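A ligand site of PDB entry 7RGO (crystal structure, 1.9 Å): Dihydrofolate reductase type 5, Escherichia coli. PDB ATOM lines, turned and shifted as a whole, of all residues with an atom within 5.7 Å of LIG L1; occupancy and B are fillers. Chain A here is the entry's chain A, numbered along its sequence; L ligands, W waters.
The side-chain carboxylate of Glu 28 sits at hydrogen-bond distance from a nitrogen (N2) of LIG L1, at 2.7 Å. O of Met 6 sits at hydrogen-bond distance from N4 of LIG L1. The side-chain amino group (NZ) of Lys 33 lies within hydrogen-bond range of an oxygen (O1) of LIG L1, 3.0 Å away. A nitrogen (N5) of LIG L1 lies within hydrogen-bond range of the side-chain amide oxygen of Gln 29 (3.1 Å). OH of Tyr 103 is in hydrogen-bond range of N4 of LIG L1. A nitrogen (N3) of LIG L1 lies close to the backbone NH of Ala 7 (3.5 Å). O of Ala 7 lies within hydrogen-bond range of N2 of LIG L1, 3.4 Å away. N4 of LIG L1 lies within hydrogen-bond range of O of Ser 97, at 3.5 Å. The side-chain hydroxyl of Tyr 103 is in hydrogen-bond range of an oxygen (O14) of LG2 L2 (3.0 Å). The backbone NH of Ala 8 is in hydrogen-bond range of an oxygen (O14) of LG2 L2, at 2.9 Å. O of Ala 8 lies within hydrogen-bond range of N7 of LG2 L2, 2.7 Å away. The backbone NH (N) of Thr 47 is in hydrogen-bond range of an oxygen (O2) of LG2 L2 (3.0 Å). The side-chain hydroxyl of Thr 47 is in hydrogen-bond range of an oxygen (O2) of LG2 L2 (2.5 Å).
The side-chain carboxylate (OE2) of Glu 28 sits at hydrogen-bond distance from the side-chain hydroxyl (OG) of Ser 116. O of Met 6 lies within hydrogen-bond range of OH of Tyr 103 (2.8 Å). The backbone NH (N) of Met 6 sits at hydrogen-bond distance from the backbone carbonyl oxygen (O) of Val 96 (2.9 Å). OH of Tyr 103 lies within hydrogen-bond range of O of Ser 97 (3.4 Å). N of Ser 116 is in hydrogen-bond range of O of Ala 7, 3.0 Å away. The backbone NH of Ala 7 is in hydrogen-bond range of the backbone carbonyl oxygen of His 114 (2.9 Å). The side-chain hydroxyl of Ser 50 lies within hydrogen-bond range of the backbone carbonyl oxygen of Pro 19 (3.3 Å).
Residues that only touch LIG L1: Ala 8, Ile 21, Phe 32, Thr 47, Ser 50, Met 51, Leu 54 and Ser 116. Hydrophobic or aromatic side chains within 4 Å of LIG L1: Met 6, Ala 8, Ile 21, Phe 32, Met 51 and Leu 54. Along chain A the residues within 4 Å of LIG L1 span positions 6 to 116. The nearest printed residue that does not touch LIG L1 is His 114 (5.0 Å).
Water W1 lies within hydrogen-bond range of N2 of LIG L1 (2.9 Å), OG of Ser 116 (2.9 Å), O of His 114 (3.0 Å) and O of Ala 7 (3.2 Å).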
ATOM      1  N   MET A   6      27.906 -17.162 -35.191  1.00  0.00           N
ATOM      2  CA  MET A   6      27.576 -18.525 -34.765  1.00  0.00           C
ATOM      3  C   MET A   6      26.115 -18.598 -34.377  1.00  0.00           C
ATOM      4  O   MET A   6      25.690 -17.876 -33.464  1.00  0.00           O
ATOM      5  CB  MET A   6      28.311 -18.971 -33.498  1.00  0.00           C
ATOM      6  CG  MET A   6      28.353 -20.488 -33.300  1.00  0.00           C
ATOM      7  SD  MET A   6      29.899 -21.239 -32.767  1.00  0.00           S
ATOM      8  CE  MET A   6      29.467 -22.975 -33.082  1.00  0.00           C
ATOM      9  N   ALA A   7      25.379 -19.545 -34.973  1.00  0.00           N
ATOM     10  CA  ALA A   7      23.971 -19.709 -34.645  1.00  0.00           C
ATOM     11  C   ALA A   7      23.549 -21.173 -34.809  1.00  0.00           C
ATOM     12  O   ALA A   7      24.141 -21.936 -35.565  1.00  0.00           O
ATOM     13  CB  ALA A   7      23.083 -18.803 -35.518  1.00  0.00           C
ATOM     14  N   ALA A   8      22.485 -21.538 -34.104  1.00  0.00           N
ATOM     15  CA  ALA A   8      21.809 -22.814 -34.299  1.00  0.00           C
ATOM     16  C   ALA A   8      20.368 -22.530 -34.703  1.00  0.00           C
ATOM     17  O   ALA A   8      19.681 -21.762 -34.022  1.00  0.00           O
ATOM     18  CB  ALA A   8      21.851 -23.670 -33.031  1.00  0.00           C
ATOM     19  N   PRO A  19      11.805 -16.288 -24.596  1.00  0.00           N
ATOM     20  CA  PRO A  19      13.196 -16.231 -24.144  1.00  0.00           C
ATOM     21  C   PRO A  19      13.936 -17.559 -24.184  1.00  0.00           C
ATOM     22  O   PRO A  19      15.016 -17.670 -23.587  1.00  0.00           O
ATOM     23  CB  PRO A  19      13.053 -15.747 -22.703  1.00  0.00           C
ATOM     24  CG  PRO A  19      11.792 -16.420 -22.254  1.00  0.00           C
ATOM     25  CD  PRO A  19      10.874 -16.413 -23.454  1.00  0.00           C
ATOM     26  N   ILE A  21      15.439 -21.153 -26.329  1.00  0.00           N
ATOM     27  CA  ILE A  21      15.768 -21.874 -27.559  1.00  0.00           C
ATOM     28  C   ILE A  21      15.014 -23.203 -27.524  1.00  0.00           C
ATOM     29  O   ILE A  21      15.284 -24.024 -26.639  1.00  0.00           O
ATOM     30  CB  ILE A  21      17.287 -22.095 -27.697  1.00  0.00           C
ATOM     31  CG1 ILE A  21      18.021 -20.755 -27.884  1.00  0.00           C
ATOM     32  CG2 ILE A  21      17.591 -23.015 -28.877  1.00  0.00           C
ATOM     33  CD1 ILE A  21      19.565 -20.844 -27.656  1.00  0.00           C
ATOM     34  N   GLU A  28      25.368 -30.515 -29.652  1.00  0.00           N
ATOM     35  CA  GLU A  28      25.496 -29.258 -30.394  1.00  0.00           C
ATOM     36  C   GLU A  28      26.090 -28.153 -29.544  1.00  0.00           C
ATOM     37  O   GLU A  28      26.832 -27.309 -30.060  1.00  0.00           O
ATOM     38  CB  GLU A  28      24.134 -28.816 -30.961  1.00  0.00           C
ATOM     39  CG  GLU A  28      24.266 -27.895 -32.199  1.00  0.00           C
ATOM     40  CD  GLU A  28      24.658 -26.456 -31.859  1.00  0.00           C
ATOM     41  OE1 GLU A  28      24.155 -25.915 -30.846  1.00  0.00           O
ATOM     42  OE2 GLU A  28      25.499 -25.861 -32.586  1.00  0.00           O
ATOM     43  N   GLN A  29      25.783 -28.132 -28.247  1.00  0.00           N
ATOM     44  CA  GLN A  29      26.334 -27.095 -27.391  1.00  0.00           C
ATOM     45  C   GLN A  29      27.851 -27.186 -27.287  1.00  0.00           C
ATOM     46  O   GLN A  29      28.502 -26.174 -27.017  1.00  0.00           O
ATOM     47  CB  GLN A  29      25.669 -27.178 -26.008  1.00  0.00           C
ATOM     48  CG  GLN A  29      24.214 -27.587 -26.129  1.00  0.00           C
ATOM     49  CD  GLN A  29      23.331 -27.039 -25.009  1.00  0.00           C
ATOM     50  OE1 GLN A  29      23.812 -26.782 -23.886  1.00  0.00           O
ATOM     51  NE2 GLN A  29      22.035 -26.856 -25.307  1.00  0.00           N
ATOM     52  N   LEU A  31      29.907 -27.636 -29.855  1.00  0.00           N
ATOM     53  CA  LEU A  31      30.444 -26.799 -30.921  1.00  0.00           C
ATOM     54  C   LEU A  31      30.448 -25.350 -30.490  1.00  0.00           C
ATOM     55  O   LEU A  31      31.453 -24.639 -30.656  1.00  0.00           O
ATOM     56  CB  LEU A  31      29.617 -26.946 -32.210  1.00  0.00           C
ATOM     57  CG  LEU A  31      29.690 -28.203 -33.041  1.00  0.00           C
ATOM     58  CD1 LEU A  31      28.475 -28.242 -33.995  1.00  0.00           C
ATOM     59  CD2 LEU A  31      31.015 -28.288 -33.807  1.00  0.00           C
ATOM     60  N   PHE A  32      29.328 -24.896 -29.955  1.00  0.00           N
ATOM     61  CA  PHE A  32      29.206 -23.513 -29.521  1.00  0.00           C
ATOM     62  C   PHE A  32      30.255 -23.178 -28.451  1.00  0.00           C
ATOM     63  O   PHE A  32      30.944 -22.154 -28.534  1.00  0.00           O
ATOM     64  CB  PHE A  32      27.789 -23.249 -29.009  1.00  0.00           C
ATOM     65  CG  PHE A  32      27.606 -21.889 -28.395  1.00  0.00           C
ATOM     66  CD1 PHE A  32      27.636 -20.744 -29.207  1.00  0.00           C
ATOM     67  CD2 PHE A  32      27.392 -21.740 -27.030  1.00  0.00           C
ATOM     68  CE1 PHE A  32      27.464 -19.477 -28.658  1.00  0.00           C
ATOM     69  CE2 PHE A  32      27.232 -20.469 -26.473  1.00  0.00           C
ATOM     70  CZ  PHE A  32      27.270 -19.334 -27.290  1.00  0.00           C
ATOM     71  N   LYS A  33      30.391 -24.044 -27.450  1.00  0.00           N
ATOM     72  CA  LYS A  33      31.407 -23.796 -26.416  1.00  0.00           C
ATOM     73  C   LYS A  33      32.817 -23.845 -27.018  1.00  0.00           C
ATOM     74  O   LYS A  33      33.638 -22.959 -26.736  1.00  0.00           O
ATOM     75  CB  LYS A  33      31.271 -24.806 -25.274  1.00  0.00           C
ATOM     76  CG  LYS A  33      29.938 -24.749 -24.508  1.00  0.00           C
ATOM     77  CD  LYS A  33      29.722 -23.377 -23.855  1.00  0.00           C
ATOM     78  CE  LYS A  33      30.346 -23.299 -22.457  1.00  0.00           C
ATOM     79  NZ  LYS A  33      30.104 -24.511 -21.623  1.00  0.00           N
ATOM     80  N   VAL A  43      26.504  -9.865 -28.453  1.00  0.00           N
ATOM     81  CA  VAL A  43      25.125 -10.292 -28.307  1.00  0.00           C
ATOM     82  C   VAL A  43      24.199  -9.118 -28.002  1.00  0.00           C
ATOM     83  O   VAL A  43      24.614  -8.082 -27.482  1.00  0.00           O
ATOM     84  CB  VAL A  43      24.964 -11.370 -27.208  1.00  0.00           C
ATOM     85  CG1 VAL A  43      25.486 -12.706 -27.707  1.00  0.00           C
ATOM     86  CG2 VAL A  43      25.684 -10.924 -25.946  1.00  0.00           C
ATOM     87  N   THR A  47      19.437 -11.671 -25.369  1.00  0.00           N
ATOM     88  CA  THR A  47      20.252 -12.873 -25.364  1.00  0.00           C
ATOM     89  C   THR A  47      21.197 -12.867 -24.183  1.00  0.00           C
ATOM     90  O   THR A  47      21.328 -13.877 -23.481  1.00  0.00           O
ATOM     91  CB  THR A  47      20.995 -12.997 -26.692  1.00  0.00           C
ATOM     92  OG1 THR A  47      20.043 -13.214 -27.743  1.00  0.00           O
ATOM     93  CG2 THR A  47      22.009 -14.148 -26.647  1.00  0.00           C
ATOM     94  N   SER A  50      19.495 -13.956 -21.104  1.00  0.00           N
ATOM     95  CA  SER A  50      19.112 -15.377 -21.059  1.00  0.00           C
ATOM     96  C   SER A  50      20.314 -16.294 -20.855  1.00  0.00           C
ATOM     97  O   SER A  50      20.211 -17.330 -20.200  1.00  0.00           O
ATOM     98  CB  SER A  50      18.405 -15.791 -22.356  1.00  0.00           C
ATOM     99  OG  SER A  50      17.062 -15.359 -22.351  1.00  0.00           O
ATOM    100  N   MET A  51      21.444 -15.947 -21.466  1.00  0.00           N
ATOM    101  CA  MET A  51      22.634 -16.782 -21.388  1.00  0.00           C
ATOM    102  C   MET A  51      23.446 -16.460 -20.145  1.00  0.00           C
ATOM    103  O   MET A  51      23.922 -17.384 -19.467  1.00  0.00           O
ATOM    104  CB  MET A  51      23.478 -16.580 -22.651  1.00  0.00           C
ATOM    105  CG  MET A  51      24.915 -17.076 -22.549  1.00  0.00           C
ATOM    106  SD  MET A  51      25.903 -16.530 -23.963  1.00  0.00           S
ATOM    107  CE  MET A  51      25.584 -14.768 -23.884  1.00  0.00           C
ATOM    108  N   LEU A  54      28.799 -16.256 -19.213  1.00  0.00           N
ATOM    109  CA  LEU A  54      29.433 -17.555 -19.018  1.00  0.00           C
ATOM    110  C   LEU A  54      30.943 -17.399 -18.849  1.00  0.00           C
ATOM    111  O   LEU A  54      31.546 -16.476 -19.406  1.00  0.00           O
ATOM    112  CB  LEU A  54      29.152 -18.496 -20.197  1.00  0.00           C
ATOM    113  CG  LEU A  54      27.700 -18.741 -20.618  1.00  0.00           C
ATOM    114  CD1 LEU A  54      27.649 -19.853 -21.692  1.00  0.00           C
ATOM    115  CD2 LEU A  54      26.827 -19.059 -19.403  1.00  0.00           C
ATOM    116  N   VAL A  96      29.574 -12.966 -33.369  1.00  0.00           N
ATOM    117  CA  VAL A  96      28.179 -12.632 -33.108  1.00  0.00           C
ATOM    118  C   VAL A  96      27.429 -13.897 -32.706  1.00  0.00           C
ATOM    119  O   VAL A  96      27.385 -14.880 -33.451  1.00  0.00           O
ATOM    120  CB  VAL A  96      27.537 -12.007 -34.346  1.00  0.00           C
ATOM    121  CG1 VAL A  96      26.043 -11.799 -34.111  1.00  0.00           C
ATOM    122  CG2 VAL A  96      28.252 -10.693 -34.690  1.00  0.00           C
ATOM    123  N   SER A  97      26.794 -13.860 -31.526  1.00  0.00           N
ATOM    124  CA  SER A  97      26.201 -15.059 -30.960  1.00  0.00           C
ATOM    125  C   SER A  97      24.723 -14.877 -30.658  1.00  0.00           C
ATOM    126  O   SER A  97      24.116 -15.737 -30.004  1.00  0.00           O
ATOM    127  CB  SER A  97      26.976 -15.488 -29.718  1.00  0.00           C
ATOM    128  OG  SER A  97      28.337 -15.658 -30.069  1.00  0.00           O
ATOM    129  N   GLY A  98      24.150 -13.793 -31.106  1.00  0.00           N
ATOM    130  CA  GLY A  98      22.735 -13.927 -31.301  1.00  0.00           C
ATOM    131  C   GLY A  98      21.939 -12.859 -30.619  1.00  0.00           C
ATOM    132  O   GLY A  98      22.489 -11.864 -30.096  1.00  0.00           O
ATOM    133  N   TYR A 103      21.417 -10.830 -35.229  1.00  0.00           N
ATOM    134  CA  TYR A 103      21.755 -11.583 -36.442  1.00  0.00           C
ATOM    135  C   TYR A 103      21.377 -10.788 -37.701  1.00  0.00           C
ATOM    136  O   TYR A 103      22.193 -10.632 -38.608  1.00  0.00           O
ATOM    137  CB  TYR A 103      21.039 -12.940 -36.444  1.00  0.00           C
ATOM    138  CG  TYR A 103      21.595 -14.009 -35.500  1.00  0.00           C
ATOM    139  CD1 TYR A 103      22.978 -14.146 -35.281  1.00  0.00           C
ATOM    140  CD2 TYR A 103      20.737 -14.905 -34.866  1.00  0.00           C
ATOM    141  CE1 TYR A 103      23.470 -15.153 -34.432  1.00  0.00           C
ATOM    142  CE2 TYR A 103      21.221 -15.910 -34.032  1.00  0.00           C
ATOM    143  CZ  TYR A 103      22.577 -16.031 -33.810  1.00  0.00           C
ATOM    144  OH  TYR A 103      23.019 -17.030 -32.960  1.00  0.00           O
ATOM    145  N   HIS A 114      29.087 -19.870 -38.729  1.00  0.00           N
ATOM    146  CA  HIS A 114      29.062 -21.181 -38.094  1.00  0.00           C
ATOM    147  C   HIS A 114      27.599 -21.516 -37.899  1.00  0.00           C
ATOM    148  O   HIS A 114      26.932 -20.920 -37.043  1.00  0.00           O
ATOM    149  CB  HIS A 114      29.822 -21.131 -36.764  1.00  0.00           C
ATOM    150  CG  HIS A 114      31.301 -20.978 -36.934  1.00  0.00           C
ATOM    151  ND1 HIS A 114      32.161 -22.049 -37.060  1.00  0.00           N
ATOM    152  CD2 HIS A 114      32.064 -19.867 -37.063  1.00  0.00           C
ATOM    153  CE1 HIS A 114      33.391 -21.598 -37.216  1.00  0.00           C
ATOM    154  NE2 HIS A 114      33.360 -20.280 -37.224  1.00  0.00           N
ATOM    155  N   SER A 116      24.657 -24.328 -37.349  1.00  0.00           N
ATOM    156  CA  SER A 116      24.170 -25.652 -37.007  1.00  0.00           C
ATOM    157  C   SER A 116      22.674 -25.682 -37.309  1.00  0.00           C
ATOM    158  O   SER A 116      21.917 -24.844 -36.817  1.00  0.00           O
ATOM    159  CB  SER A 116      24.417 -25.982 -35.523  1.00  0.00           C
ATOM    160  OG  SER A 116      25.805 -26.038 -35.229  1.00  0.00           O
HETATM  161  C1  LIG L   1      22.324 -19.032 -25.603  1.00  0.00           C
HETATM  162  C2  LIG L   1      23.477 -20.200 -28.740  1.00  0.00           C
HETATM  163  C3  LIG L   1      24.058 -20.995 -29.809  1.00  0.00           C
HETATM  164  C4  LIG L   1      23.018 -19.476 -27.881  1.00  0.00           C
HETATM  165  C5  LIG L   1      22.523 -18.472 -26.899  1.00  0.00           C
HETATM  166  C6  LIG L   1      24.299 -23.971 -27.953  1.00  0.00           C
HETATM  167  C7  LIG L   1      23.356 -23.009 -28.672  1.00  0.00           C
HETATM  168  C8  LIG L   1      23.998 -22.388 -29.750  1.00  0.00           C
HETATM  169  C9  LIG L   1      25.154 -22.488 -31.788  1.00  0.00           C
HETATM  170  C10 LIG L   1      24.705 -20.391 -30.886  1.00  0.00           C
HETATM  171  C11 LIG L   1      23.229 -19.948 -25.054  1.00  0.00           C
HETATM  172  C12 LIG L   1      23.024 -20.462 -23.761  1.00  0.00           C
HETATM  173  C13 LIG L   1      23.895 -21.420 -23.207  1.00  0.00           C
HETATM  174  C14 LIG L   1      24.514 -22.341 -24.052  1.00  0.00           C
HETATM  175  C15 LIG L   1      25.360 -23.336 -23.556  1.00  0.00           C
HETATM  176  C16 LIG L   1      25.574 -23.436 -22.173  1.00  0.00           C
HETATM  177  C17 LIG L   1      26.402 -24.456 -21.678  1.00  0.00           C
HETATM  178  C18 LIG L   1      24.949 -22.528 -21.314  1.00  0.00           C
HETATM  179  C19 LIG L   1      24.095 -21.530 -21.825  1.00  0.00           C
HETATM  180  C20 LIG L   1      21.900 -20.084 -23.045  1.00  0.00           C
HETATM  181  C21 LIG L   1      20.990 -19.173 -23.572  1.00  0.00           C
HETATM  182  C22 LIG L   1      21.207 -18.648 -24.850  1.00  0.00           C
HETATM  183  C23 LIG L   1      23.609 -17.382 -26.805  1.00  0.00           C
HETATM  184  N1  LIG L   1      24.550 -23.106 -30.748  1.00  0.00           N
HETATM  185  N2  LIG L   1      25.689 -23.223 -32.766  1.00  0.00           N
HETATM  186  N3  LIG L   1      25.235 -21.139 -31.864  1.00  0.00           N
HETATM  187  N4  LIG L   1      24.761 -19.041 -30.929  1.00  0.00           N
HETATM  188  N5  LIG L   1      26.130 -25.697 -22.157  1.00  0.00           N
HETATM  189  O1  LIG L   1      27.277 -24.197 -20.831  1.00  0.00           O
HETATM  190 CL1  LIG L   1      20.084 -17.519 -25.491  1.00  0.00          CL
HETATM  191  P1  LG2 L   2      18.392  -9.887 -29.020  1.00  0.00           P
HETATM  192  O1  LG2 L   2      18.859  -9.728 -30.401  1.00  0.00           O
HETATM  193  O2  LG2 L   2      19.116 -10.906 -28.202  1.00  0.00           O
HETATM  194  O3  LG2 L   2      18.433  -8.459 -28.270  1.00  0.00           O
HETATM  195  C1  LG2 L   2      17.704  -7.366 -28.787  1.00  0.00           C
HETATM  196  C2  LG2 L   2      18.081  -6.172 -27.930  1.00  0.00           C
HETATM  197  O4  LG2 L   2      19.423  -5.772 -28.171  1.00  0.00           O
HETATM  198  C3  LG2 L   2      17.237  -4.936 -28.196  1.00  0.00           C
HETATM  199  O5  LG2 L   2      16.052  -5.020 -27.441  1.00  0.00           O
HETATM  200  C4  LG2 L   2      18.168  -3.822 -27.736  1.00  0.00           C
HETATM  201  O6  LG2 L   2      18.277  -3.808 -26.335  1.00  0.00           O
HETATM  202  C5  LG2 L   2      19.512  -4.365 -28.177  1.00  0.00           C
HETATM  203  N1  LG2 L   2      19.846  -3.907 -29.538  1.00  0.00           N
HETATM  204  C6  LG2 L   2      19.578  -4.564 -30.724  1.00  0.00           C
HETATM  205  N2  LG2 L   2      20.089  -3.828 -31.738  1.00  0.00           N
HETATM  206  C7  LG2 L   2      20.690  -2.730 -31.214  1.00  0.00           C
HETATM  207  C8  LG2 L   2      21.373  -1.655 -31.785  1.00  0.00           C
HETATM  208  N3  LG2 L   2      21.538  -1.566 -33.111  1.00  0.00           N
HETATM  209  N4  LG2 L   2      21.883  -0.672 -30.981  1.00  0.00           N
HETATM  210  C9  LG2 L   2      21.727  -0.748 -29.612  1.00  0.00           C
HETATM  211  N5  LG2 L   2      21.050  -1.803 -29.035  1.00  0.00           N
HETATM  212  C10 LG2 L   2      20.541  -2.778 -29.832  1.00  0.00           C
HETATM  213  O7  LG2 L   2      16.809 -10.195 -28.975  1.00  0.00           O
HETATM  214  P2  LG2 L   2      15.826 -11.079 -29.880  1.00  0.00           P
HETATM  215  O8  LG2 L   2      14.515 -11.148 -29.176  1.00  0.00           O
HETATM  216  O9  LG2 L   2      15.898 -10.638 -31.292  1.00  0.00           O
HETATM  217  O10 LG2 L   2      16.480 -12.549 -29.830  1.00  0.00           O
HETATM  218  C11 LG2 L   2      16.382 -13.312 -28.647  1.00  0.00           C
HETATM  219  C12 LG2 L   2      15.840 -14.676 -29.036  1.00  0.00           C
HETATM  220  O11 LG2 L   2      16.799 -15.360 -29.841  1.00  0.00           O
HETATM  221  C13 LG2 L   2      15.608 -15.552 -27.813  1.00  0.00           C
HETATM  222  O12 LG2 L   2      14.481 -16.360 -28.075  1.00  0.00           O
HETATM  223  C14 LG2 L   2      16.811 -16.450 -27.745  1.00  0.00           C
HETATM  224  O13 LG2 L   2      16.455 -17.707 -27.192  1.00  0.00           O
HETATM  225  C15 LG2 L   2      17.124 -16.601 -29.227  1.00  0.00           C
HETATM  226  N6  LG2 L   2      18.521 -16.944 -29.522  1.00  0.00           N
HETATM  227  C16 LG2 L   2      18.761 -18.044 -30.300  1.00  0.00           C
HETATM  228  C17 LG2 L   2      20.057 -18.385 -30.622  1.00  0.00           C
HETATM  229  C18 LG2 L   2      20.311 -19.558 -31.515  1.00  0.00           C
HETATM  230  O14 LG2 L   2      21.530 -19.535 -32.185  1.00  0.00           O
HETATM  231  N7  LG2 L   2      19.434 -20.565 -31.647  1.00  0.00           N
HETATM  232  C19 LG2 L   2      21.134 -17.597 -30.185  1.00  0.00           C
HETATM  233  C20 LG2 L   2      20.857 -16.478 -29.405  1.00  0.00           C
HETATM  234  C21 LG2 L   2      19.548 -16.148 -29.085  1.00  0.00           C
HETATM  235  P3  LG2 L   2      17.329  -2.948 -25.367  1.00  0.00           P
HETATM  236  O15 LG2 L   2      15.962  -3.595 -25.345  1.00  0.00           O
HETATM  237  O16 LG2 L   2      17.943  -3.014 -23.991  1.00  0.00           O
HETATM  238  O17 LG2 L   2      17.308  -1.523 -25.864  1.00  0.00           O
HETATM  239  O   HOH W   1      27.029 -23.359 -35.338  1.00  0.00           O
